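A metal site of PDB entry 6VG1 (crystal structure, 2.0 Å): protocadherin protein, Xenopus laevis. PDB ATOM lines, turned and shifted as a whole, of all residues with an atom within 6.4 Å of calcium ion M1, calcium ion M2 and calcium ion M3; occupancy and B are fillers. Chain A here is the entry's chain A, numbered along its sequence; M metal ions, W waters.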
ATOM      1  N   GLU A   9      26.586 -19.011  26.518  1.00  0.00           N
ATOM      2  CA  GLU A   9      27.590 -17.976  26.712  1.00  0.00           C
ATOM      3  C   GLU A   9      27.222 -17.064  27.881  1.00  0.00           C
ATOM      4  O   GLU A   9      26.058 -16.974  28.273  1.00  0.00           O
ATOM      5  CB  GLU A   9      27.769 -17.144  25.432  1.00  0.00           C
ATOM      6  CG  GLU A   9      26.600 -16.256  25.073  1.00  0.00           C
ATOM      7  CD  GLU A   9      26.951 -15.204  24.030  1.00  0.00           C
ATOM      8  OE1 GLU A   9      28.067 -14.632  24.112  1.00  0.00           O
ATOM      9  OE2 GLU A   9      26.130 -14.943  23.118  1.00  0.00           O
ATOM     10  N   GLU A  10      28.227 -16.401  28.452  1.00  0.00           N
ATOM     11  CA  GLU A  10      28.037 -15.450  29.541  1.00  0.00           C
ATOM     12  C   GLU A  10      27.258 -16.073  30.706  1.00  0.00           C
ATOM     13  O   GLU A  10      26.435 -15.414  31.342  1.00  0.00           O
ATOM     14  CB  GLU A  10      27.325 -14.180  29.061  1.00  0.00           C
ATOM     15  CG  GLU A  10      27.687 -13.678  27.680  1.00  0.00           C
ATOM     16  CD  GLU A  10      28.644 -12.484  27.702  1.00  0.00           C
ATOM     17  OE1 GLU A  10      29.308 -12.258  28.728  1.00  0.00           O
ATOM     18  OE2 GLU A  10      28.719 -11.788  26.665  1.00  0.00           O
ATOM     19  N   ARG A  57      34.672 -15.755  32.308  1.00  0.00           N
ATOM     20  CA  ARG A  57      33.588 -15.279  31.459  1.00  0.00           C
ATOM     21  C   ARG A  57      33.720 -15.847  30.058  1.00  0.00           C
ATOM     22  O   ARG A  57      34.821 -15.887  29.491  1.00  0.00           O
ATOM     23  CB  ARG A  57      33.618 -13.760  31.436  1.00  0.00           C
ATOM     24  CG  ARG A  57      32.545 -13.093  30.612  1.00  0.00           C
ATOM     25  CD  ARG A  57      32.725 -11.578  30.710  1.00  0.00           C
ATOM     26  NE  ARG A  57      31.746 -10.826  29.934  1.00  0.00           N
ATOM     27  CZ  ARG A  57      31.921 -10.480  28.669  1.00  0.00           C
ATOM     28  NH1 ARG A  57      33.023 -10.814  28.019  1.00  0.00           N
ATOM     29  NH2 ARG A  57      30.983  -9.779  28.041  1.00  0.00           N
ATOM     30  N   ILE A  58      32.602 -16.291  29.497  1.00  0.00           N
ATOM     31  CA  ILE A  58      32.567 -16.875  28.159  1.00  0.00           C
ATOM     32  C   ILE A  58      31.682 -16.000  27.274  1.00  0.00           C
ATOM     33  O   ILE A  58      30.454 -16.057  27.389  1.00  0.00           O
ATOM     34  CB  ILE A  58      32.060 -18.318  28.161  1.00  0.00           C
ATOM     35  CG1 ILE A  58      32.976 -19.217  28.983  1.00  0.00           C
ATOM     36  CG2 ILE A  58      31.934 -18.834  26.729  1.00  0.00           C
ATOM     37  CD1 ILE A  58      32.424 -20.620  29.190  1.00  0.00           C
ATOM     38  N   ASP A  59      32.304 -15.208  26.394  1.00  0.00           N
ATOM     39  CA  ASP A  59      31.580 -14.328  25.474  1.00  0.00           C
ATOM     40  C   ASP A  59      31.729 -14.862  24.058  1.00  0.00           C
ATOM     41  O   ASP A  59      32.798 -14.743  23.452  1.00  0.00           O
ATOM     42  CB  ASP A  59      32.109 -12.898  25.580  1.00  0.00           C
ATOM     43  CG  ASP A  59      31.282 -11.905  24.768  1.00  0.00           C
ATOM     44  OD1 ASP A  59      30.281 -12.321  24.143  1.00  0.00           O
ATOM     45  OD2 ASP A  59      31.628 -10.706  24.761  1.00  0.00           O
ATOM     46  N   ARG A  60      30.639 -15.413  23.518  1.00  0.00           N
ATOM     47  CA  ARG A  60      30.703 -15.996  22.175  1.00  0.00           C
ATOM     48  C   ARG A  60      31.138 -14.956  21.147  1.00  0.00           C
ATOM     49  O   ARG A  60      31.991 -15.225  20.301  1.00  0.00           O
ATOM     50  CB  ARG A  60      29.353 -16.590  21.790  1.00  0.00           C
ATOM     51  CG  ARG A  60      29.444 -17.636  20.683  1.00  0.00           C
ATOM     52  CD  ARG A  60      28.198 -17.690  19.832  1.00  0.00           C
ATOM     53  NE  ARG A  60      27.856 -16.363  19.308  1.00  0.00           N
ATOM     54  CZ  ARG A  60      28.572 -15.703  18.401  1.00  0.00           C
ATOM     55  NH1 ARG A  60      29.679 -16.247  17.917  1.00  0.00           N
ATOM     56  NH2 ARG A  60      28.177 -14.515  17.986  1.00  0.00           N
ATOM     57  N   GLU A  61      30.550 -13.765  21.200  1.00  0.00           N
ATOM     58  CA  GLU A  61      30.857 -12.730  20.221  1.00  0.00           C
ATOM     59  C   GLU A  61      32.326 -12.302  20.255  1.00  0.00           C
ATOM     60  O   GLU A  61      32.781 -11.655  19.303  1.00  0.00           O
ATOM     61  CB  GLU A  61      29.948 -11.521  20.444  1.00  0.00           C
ATOM     62  CG  GLU A  61      28.505 -11.692  19.928  1.00  0.00           C
ATOM     63  CD  GLU A  61      27.589 -12.415  20.892  1.00  0.00           C
ATOM     64  OE1 GLU A  61      27.567 -12.077  22.094  1.00  0.00           O
ATOM     65  OE2 GLU A  61      26.872 -13.330  20.443  1.00  0.00           O
ATOM     66  N   ARG A  62      33.076 -12.661  21.300  1.00  0.00           N
ATOM     67  CA  ARG A  62      34.486 -12.314  21.395  1.00  0.00           C
ATOM     68  C   ARG A  62      35.408 -13.429  20.933  1.00  0.00           C
ATOM     69  O   ARG A  62      36.530 -13.149  20.505  1.00  0.00           O
ATOM     70  CB  ARG A  62      34.850 -11.931  22.830  1.00  0.00           C
ATOM     71  CG  ARG A  62      36.331 -11.655  23.033  1.00  0.00           C
ATOM     72  CD  ARG A  62      36.631 -11.184  24.457  1.00  0.00           C
ATOM     73  NE  ARG A  62      36.256 -12.187  25.455  1.00  0.00           N
ATOM     74  CZ  ARG A  62      37.008 -13.225  25.799  1.00  0.00           C
ATOM     75  NH1 ARG A  62      38.181 -13.420  25.214  1.00  0.00           N
ATOM     76  NH2 ARG A  62      36.582 -14.077  26.717  1.00  0.00           N
ATOM     77  N   ASP A  95      24.479 -19.421  21.503  1.00  0.00           N
ATOM     78  CA  ASP A  95      24.437 -17.971  21.379  1.00  0.00           C
ATOM     79  C   ASP A  95      23.257 -17.410  22.171  1.00  0.00           C
ATOM     80  O   ASP A  95      22.161 -17.972  22.161  1.00  0.00           O
ATOM     81  CB  ASP A  95      24.328 -17.554  19.916  1.00  0.00           C
ATOM     82  CG  ASP A  95      24.192 -16.049  19.738  1.00  0.00           C
ATOM     83  OD1 ASP A  95      24.332 -15.294  20.726  1.00  0.00           O
ATOM     84  OD2 ASP A  95      23.940 -15.605  18.595  1.00  0.00           O
ATOM     85  N   ILE A  96      23.505 -16.275  22.841  1.00  0.00           N
ATOM     86  CA  ILE A  96      22.478 -15.528  23.552  1.00  0.00           C
ATOM     87  C   ILE A  96      22.295 -14.204  22.835  1.00  0.00           C
ATOM     88  O   ILE A  96      23.217 -13.703  22.181  1.00  0.00           O
ATOM     89  CB  ILE A  96      22.847 -15.340  25.031  1.00  0.00           C
ATOM     90  CG1 ILE A  96      21.589 -15.128  25.874  1.00  0.00           C
ATOM     91  CG2 ILE A  96      23.784 -14.162  25.219  1.00  0.00           C
ATOM     92  CD1 ILE A  96      20.682 -16.350  25.941  1.00  0.00           C
ATOM     93  N   ASN A  97      21.096 -13.635  22.965  1.00  0.00           N
ATOM     94  CA  ASN A  97      20.723 -12.426  22.229  1.00  0.00           C
ATOM     95  C   ASN A  97      21.069 -11.160  23.021  1.00  0.00           C
ATOM     96  O   ASN A  97      20.238 -10.282  23.243  1.00  0.00           O
ATOM     97  CB  ASN A  97      19.237 -12.486  21.914  1.00  0.00           C
ATOM     98  CG  ASN A  97      18.817 -11.437  20.896  1.00  0.00           C
ATOM     99  OD1 ASN A  97      19.616 -11.022  20.051  1.00  0.00           O
ATOM    100  ND2 ASN A  97      17.568 -11.002  20.980  1.00  0.00           N
ATOM    101  N   ASP A  98      22.328 -11.077  23.440  1.00  0.00           N
ATOM    102  CA  ASP A  98      22.817  -9.951  24.227  1.00  0.00           C
ATOM    103  C   ASP A  98      23.378  -8.837  23.363  1.00  0.00           C
ATOM    104  O   ASP A  98      24.103  -7.983  23.868  1.00  0.00           O
ATOM    105  CB  ASP A  98      23.884 -10.425  25.224  1.00  0.00           C
ATOM    106  CG  ASP A  98      24.974 -11.277  24.572  1.00  0.00           C
ATOM    107  OD1 ASP A  98      24.885 -11.570  23.357  1.00  0.00           O
ATOM    108  OD2 ASP A  98      25.913 -11.665  25.299  1.00  0.00           O
ATOM    109  N   ASN A  99      23.042  -8.819  22.076  1.00  0.00           N
ATOM    110  CA  ASN A  99      23.451  -7.736  21.197  1.00  0.00           C
ATOM    111  C   ASN A  99      22.290  -7.361  20.304  1.00  0.00           C
ATOM    112  O   ASN A  99      21.606  -8.237  19.745  1.00  0.00           O
ATOM    113  CB  ASN A  99      24.665  -8.115  20.351  1.00  0.00           C
ATOM    114  CG  ASN A  99      25.962  -8.013  21.123  1.00  0.00           C
ATOM    115  OD1 ASN A  99      26.335  -6.927  21.584  1.00  0.00           O
ATOM    116  ND2 ASN A  99      26.654  -9.125  21.291  1.00  0.00           N
ATOM    117  N   SER A 100      22.088  -6.043  20.152  1.00  0.00           N
ATOM    118  CA  SER A 100      21.002  -5.483  19.397  1.00  0.00           C
ATOM    119  C   SER A 100      21.510  -4.885  18.101  1.00  0.00           C
ATOM    120  O   SER A 100      22.658  -4.441  18.022  1.00  0.00           O
ATOM    121  CB  SER A 100      20.324  -4.409  20.227  1.00  0.00           C
ATOM    122  OG  SER A 100      21.306  -3.596  20.870  1.00  0.00           O
ATOM    123  N   PRO A 101      20.665  -4.818  17.082  1.00  0.00           N
ATOM    124  CA  PRO A 101      21.089  -4.178  15.821  1.00  0.00           C
ATOM    125  C   PRO A 101      21.549  -2.753  16.061  1.00  0.00           C
ATOM    126  O   PRO A 101      20.959  -2.014  16.847  1.00  0.00           O
ATOM    127  CB  PRO A 101      19.835  -4.240  14.948  1.00  0.00           C
ATOM    128  CG  PRO A 101      19.038  -5.394  15.494  1.00  0.00           C
ATOM    129  CD  PRO A 101      19.304  -5.386  16.997  1.00  0.00           C
ATOM    130  N   ASP A 129      24.316  -6.698  13.796  1.00  0.00           N
ATOM    131  CA  ASP A 129      23.953  -7.374  15.040  1.00  0.00           C
ATOM    132  C   ASP A 129      25.010  -8.434  15.279  1.00  0.00           C
ATOM    133  O   ASP A 129      25.153  -9.356  14.465  1.00  0.00           O
ATOM    134  CB  ASP A 129      22.562  -7.998  14.945  1.00  0.00           C
ATOM    135  CG  ASP A 129      22.073  -8.565  16.277  1.00  0.00           C
ATOM    136  OD1 ASP A 129      22.848  -8.698  17.259  1.00  0.00           O
ATOM    137  OD2 ASP A 129      20.872  -8.920  16.324  1.00  0.00           O
ATOM    138  N   GLU A 130      25.765  -8.303  16.372  1.00  0.00           N
ATOM    139  CA  GLU A 130      26.916  -9.165  16.593  1.00  0.00           C
ATOM    140  C   GLU A 130      26.535 -10.584  17.019  1.00  0.00           C
ATOM    141  O   GLU A 130      27.443 -11.402  17.185  1.00  0.00           O
ATOM    142  CB  GLU A 130      27.842  -8.529  17.638  1.00  0.00           C
ATOM    143  CG  GLU A 130      28.526  -7.269  17.136  1.00  0.00           C
ATOM    144  CD  GLU A 130      29.635  -6.797  18.060  1.00  0.00           C
ATOM    145  OE1 GLU A 130      29.751  -7.352  19.175  1.00  0.00           O
ATOM    146  OE2 GLU A 130      30.382  -5.877  17.672  1.00  0.00           O
ATOM    147  N   ASP A 131      25.257 -10.881  17.207  1.00  0.00           N
ATOM    148  CA  ASP A 131      24.828 -12.262  17.411  1.00  0.00           C
ATOM    149  C   ASP A 131      24.818 -12.995  16.073  1.00  0.00           C
ATOM    150  O   ASP A 131      25.213 -12.439  15.035  1.00  0.00           O
ATOM    151  CB  ASP A 131      23.457 -12.274  18.079  1.00  0.00           C
ATOM    152  CG  ASP A 131      23.423 -11.452  19.362  1.00  0.00           C
ATOM    153  OD1 ASP A 131      24.408 -11.484  20.149  1.00  0.00           O
ATOM    154  OD2 ASP A 131      22.400 -10.754  19.590  1.00  0.00           O
ATOM    155  N   VAL A 132      24.381 -14.258  16.078  1.00  0.00           N
ATOM    156  CA  VAL A 132      24.312 -15.042  14.852  1.00  0.00           C
ATOM    157  C   VAL A 132      22.933 -15.693  14.749  1.00  0.00           C
ATOM    158  O   VAL A 132      22.136 -15.656  15.685  1.00  0.00           O
ATOM    159  CB  VAL A 132      25.424 -16.129  14.785  1.00  0.00           C
ATOM    160  CG1 VAL A 132      26.805 -15.493  14.759  1.00  0.00           C
ATOM    161  CG2 VAL A 132      25.289 -17.089  15.953  1.00  0.00           C
ATOM    162  N   VAL A 134      19.173 -16.675  14.195  1.00  0.00           N
ATOM    163  CA  VAL A 134      17.966 -15.873  14.373  1.00  0.00           C
ATOM    164  C   VAL A 134      18.278 -14.607  15.150  1.00  0.00           C
ATOM    165  O   VAL A 134      17.641 -13.565  14.955  1.00  0.00           O
ATOM    166  CB  VAL A 134      16.861 -16.687  15.063  1.00  0.00           C
ATOM    167  CG1 VAL A 134      16.571 -17.954  14.283  1.00  0.00           C
ATOM    168  CG2 VAL A 134      17.246 -16.986  16.513  1.00  0.00           C
ATOM    169  N   ASN A 135      19.259 -14.667  16.055  1.00  0.00           N
ATOM    170  CA  ASN A 135      19.647 -13.491  16.829  1.00  0.00           C
ATOM    171  C   ASN A 135      20.333 -12.430  15.985  1.00  0.00           C
ATOM    172  O   ASN A 135      20.661 -11.363  16.511  1.00  0.00           O
ATOM    173  CB  ASN A 135      20.545 -13.898  17.984  1.00  0.00           C
ATOM    174  CG  ASN A 135      19.811 -14.721  19.019  1.00  0.00           C
ATOM    175  OD1 ASN A 135      18.589 -14.853  18.948  1.00  0.00           O
ATOM    176  ND2 ASN A 135      20.546 -15.266  19.979  1.00  0.00           N
ATOM    177  N   SER A 136      20.537 -12.694  14.700  1.00  0.00           N
ATOM    178  CA  SER A 136      21.091 -11.712  13.773  1.00  0.00           C
ATOM    179  C   SER A 136      19.954 -10.891  13.164  1.00  0.00           C
ATOM    180  O   SER A 136      18.763 -11.160  13.387  1.00  0.00           O
ATOM    181  CB  SER A 136      21.896 -12.395  12.686  1.00  0.00           C
ATOM    182  OG  SER A 136      21.035 -13.065  11.768  1.00  0.00           O
ATOM    183  N   ILE A 137      20.307  -9.893  12.367  1.00  0.00           N
ATOM    184  CA  ILE A 137      19.310  -9.017  11.750  1.00  0.00           C
ATOM    185  C   ILE A 137      18.490  -9.828  10.759  1.00  0.00           C
ATOM    186  O   ILE A 137      19.028 -10.400   9.804  1.00  0.00           O
ATOM    187  CB  ILE A 137      19.986  -7.828  11.064  1.00  0.00           C
ATOM    188  CG1 ILE A 137      20.637  -6.932  12.123  1.00  0.00           C
ATOM    189  CG2 ILE A 137      18.974  -7.030  10.242  1.00  0.00           C
ATOM    190  CD1 ILE A 137      21.490  -5.802  11.552  1.00  0.00           C
ATOM    191  N   ASP A 186      15.918  -8.317  14.911  1.00  0.00           N
ATOM    192  CA  ASP A 186      16.353  -9.703  14.854  1.00  0.00           C
ATOM    193  C   ASP A 186      15.219 -10.646  15.265  1.00  0.00           C
ATOM    194  O   ASP A 186      14.120 -10.223  15.635  1.00  0.00           O
ATOM    195  CB  ASP A 186      17.588  -9.907  15.746  1.00  0.00           C
ATOM    196  CG  ASP A 186      17.325  -9.572  17.225  1.00  0.00           C
ATOM    197  OD1 ASP A 186      16.165  -9.697  17.687  1.00  0.00           O
ATOM    198  OD2 ASP A 186      18.287  -9.185  17.921  1.00  0.00           O
ATOM    199  N   GLY A 187      15.518 -11.951  15.228  1.00  0.00           N
ATOM    200  CA  GLY A 187      14.523 -12.968  15.495  1.00  0.00           C
ATOM    201  C   GLY A 187      14.427 -13.345  16.969  1.00  0.00           C
ATOM    202  O   GLY A 187      15.163 -12.838  17.825  1.00  0.00           O
ATOM    203  N   ARG A 192      15.147  -7.407  19.529  1.00  0.00           N
ATOM    204  CA  ARG A 192      15.881  -6.170  19.743  1.00  0.00           C
ATOM    205  C   ARG A 192      15.954  -5.398  18.433  1.00  0.00           C
ATOM    206  O   ARG A 192      16.358  -5.949  17.399  1.00  0.00           O
ATOM    207  CB  ARG A 192      17.270  -6.449  20.301  1.00  0.00           C
ATOM    208  CG  ARG A 192      17.212  -7.030  21.719  1.00  0.00           C
ATOM    209  CD  ARG A 192      18.484  -7.759  22.121  1.00  0.00           C
ATOM    210  NE  ARG A 192      19.576  -6.871  22.505  1.00  0.00           N
ATOM    211  CZ  ARG A 192      19.972  -6.666  23.755  1.00  0.00           C
ATOM    212  NH1 ARG A 192      19.372  -7.282  24.758  1.00  0.00           N
ATOM    213  NH2 ARG A 192      20.991  -5.846  23.998  1.00  0.00           N
HETATM  214 CA    CA M   1      25.118 -13.252  21.684  1.00  0.00          CA
HETATM  215 CA    CA M   2      27.891 -12.242  24.400  1.00  0.00          CA
HETATM  216 CA    CA M   3      20.698  -9.870  18.303  1.00  0.00          CA
HETATM  217  O   HOH W   1      28.920  -9.504  24.669  1.00  0.00           O
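Of the 26 residues printed, 5 come within 4 Å of calcium ion M2. The nearest printed residue that does not touch calcium ion M2 is Arg 60 (4.3 Å).
Calcium ion M3 is bound by OD2 of Asp 129 (2.2 Å), OD2 of Asp 131 (2.3 Å), O of Asn 135 (2.3 Å), OD1 of Asn 97 (2.4 Å), O of Asn 99 (2.4 Å), OD2 of Asp 186 (2.5 Å) and OD1 of Asp 129 (2.7 Å). Calcium ion M3 has seven donor atoms within binding distance.
O of Asn 97 sits close to NH1 of Arg 192, at 3.5 Å. OD2 of Asp 95 is in hydrogen-bond range of N of Val 132 (2.9 Å). OD1 of Asp 186 lies within hydrogen-bond range of N of Arg 192 (3.1 Å). N of Glu 10 sits at hydrogen-bond distance from O of Ile 58. NH2 of Arg 60 lies close to OE2 of Glu 61 (3.0 Å). The side-chain carboxylate (OD2) of Asp 59 lies within salt-bridge range of the guanidinium group (NH2) of Arg 57. The side-chain carboxylate of Glu 10 is in salt-bridge range of the guanidinium group of Arg 57 (3.1 Å). The side-chain amide nitrogen of Asn 99 lies close to the side-chain carboxylate of Glu 61 (3.2 Å).
Calcium ion M1 is bound by the backbone carbonyl oxygen (O) of Ile 96 (2.0 Å), the side-chain carboxylate (OE2) of Glu 61 (2.2 Å), the side-chain carboxylate (OD1) of Asp 98 (2.4 Å), the side-chain carboxylate (OD1) of Asp 95 (2.4 Å), the side-chain carboxylate (OE2) of Glu 9 (2.4 Å), the side-chain carboxylate (OD1) of Asp 131 (2.4 Å) and the side-chain carboxylate (OE1) of Glu 61 (2.7 Å). Calcium ion M1 has seven donor atoms within binding distance.
Six residues have an atom within 4 Å of calcium ion M1: Glu 9, Glu 61, Asp 95, Ile 96, Asp 98 and Asp 131.
Of the 26 residues printed, 6 come within 4 Å of calcium ion M3.
Calcium ion M2 is bound by OD2 of Asp 98 (2.2 Å), OE1 of Glu 61 (2.3 Å), OD1 of Asp 59 (2.4 Å), OE1 of Glu 9 (2.4 Å) and OE2 of Glu 10 (2.5 Å). Calcium ion M2 has five donor atoms within binding distance. Slightly farther from calcium ion M2 lies water W1 (2.9 Å).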
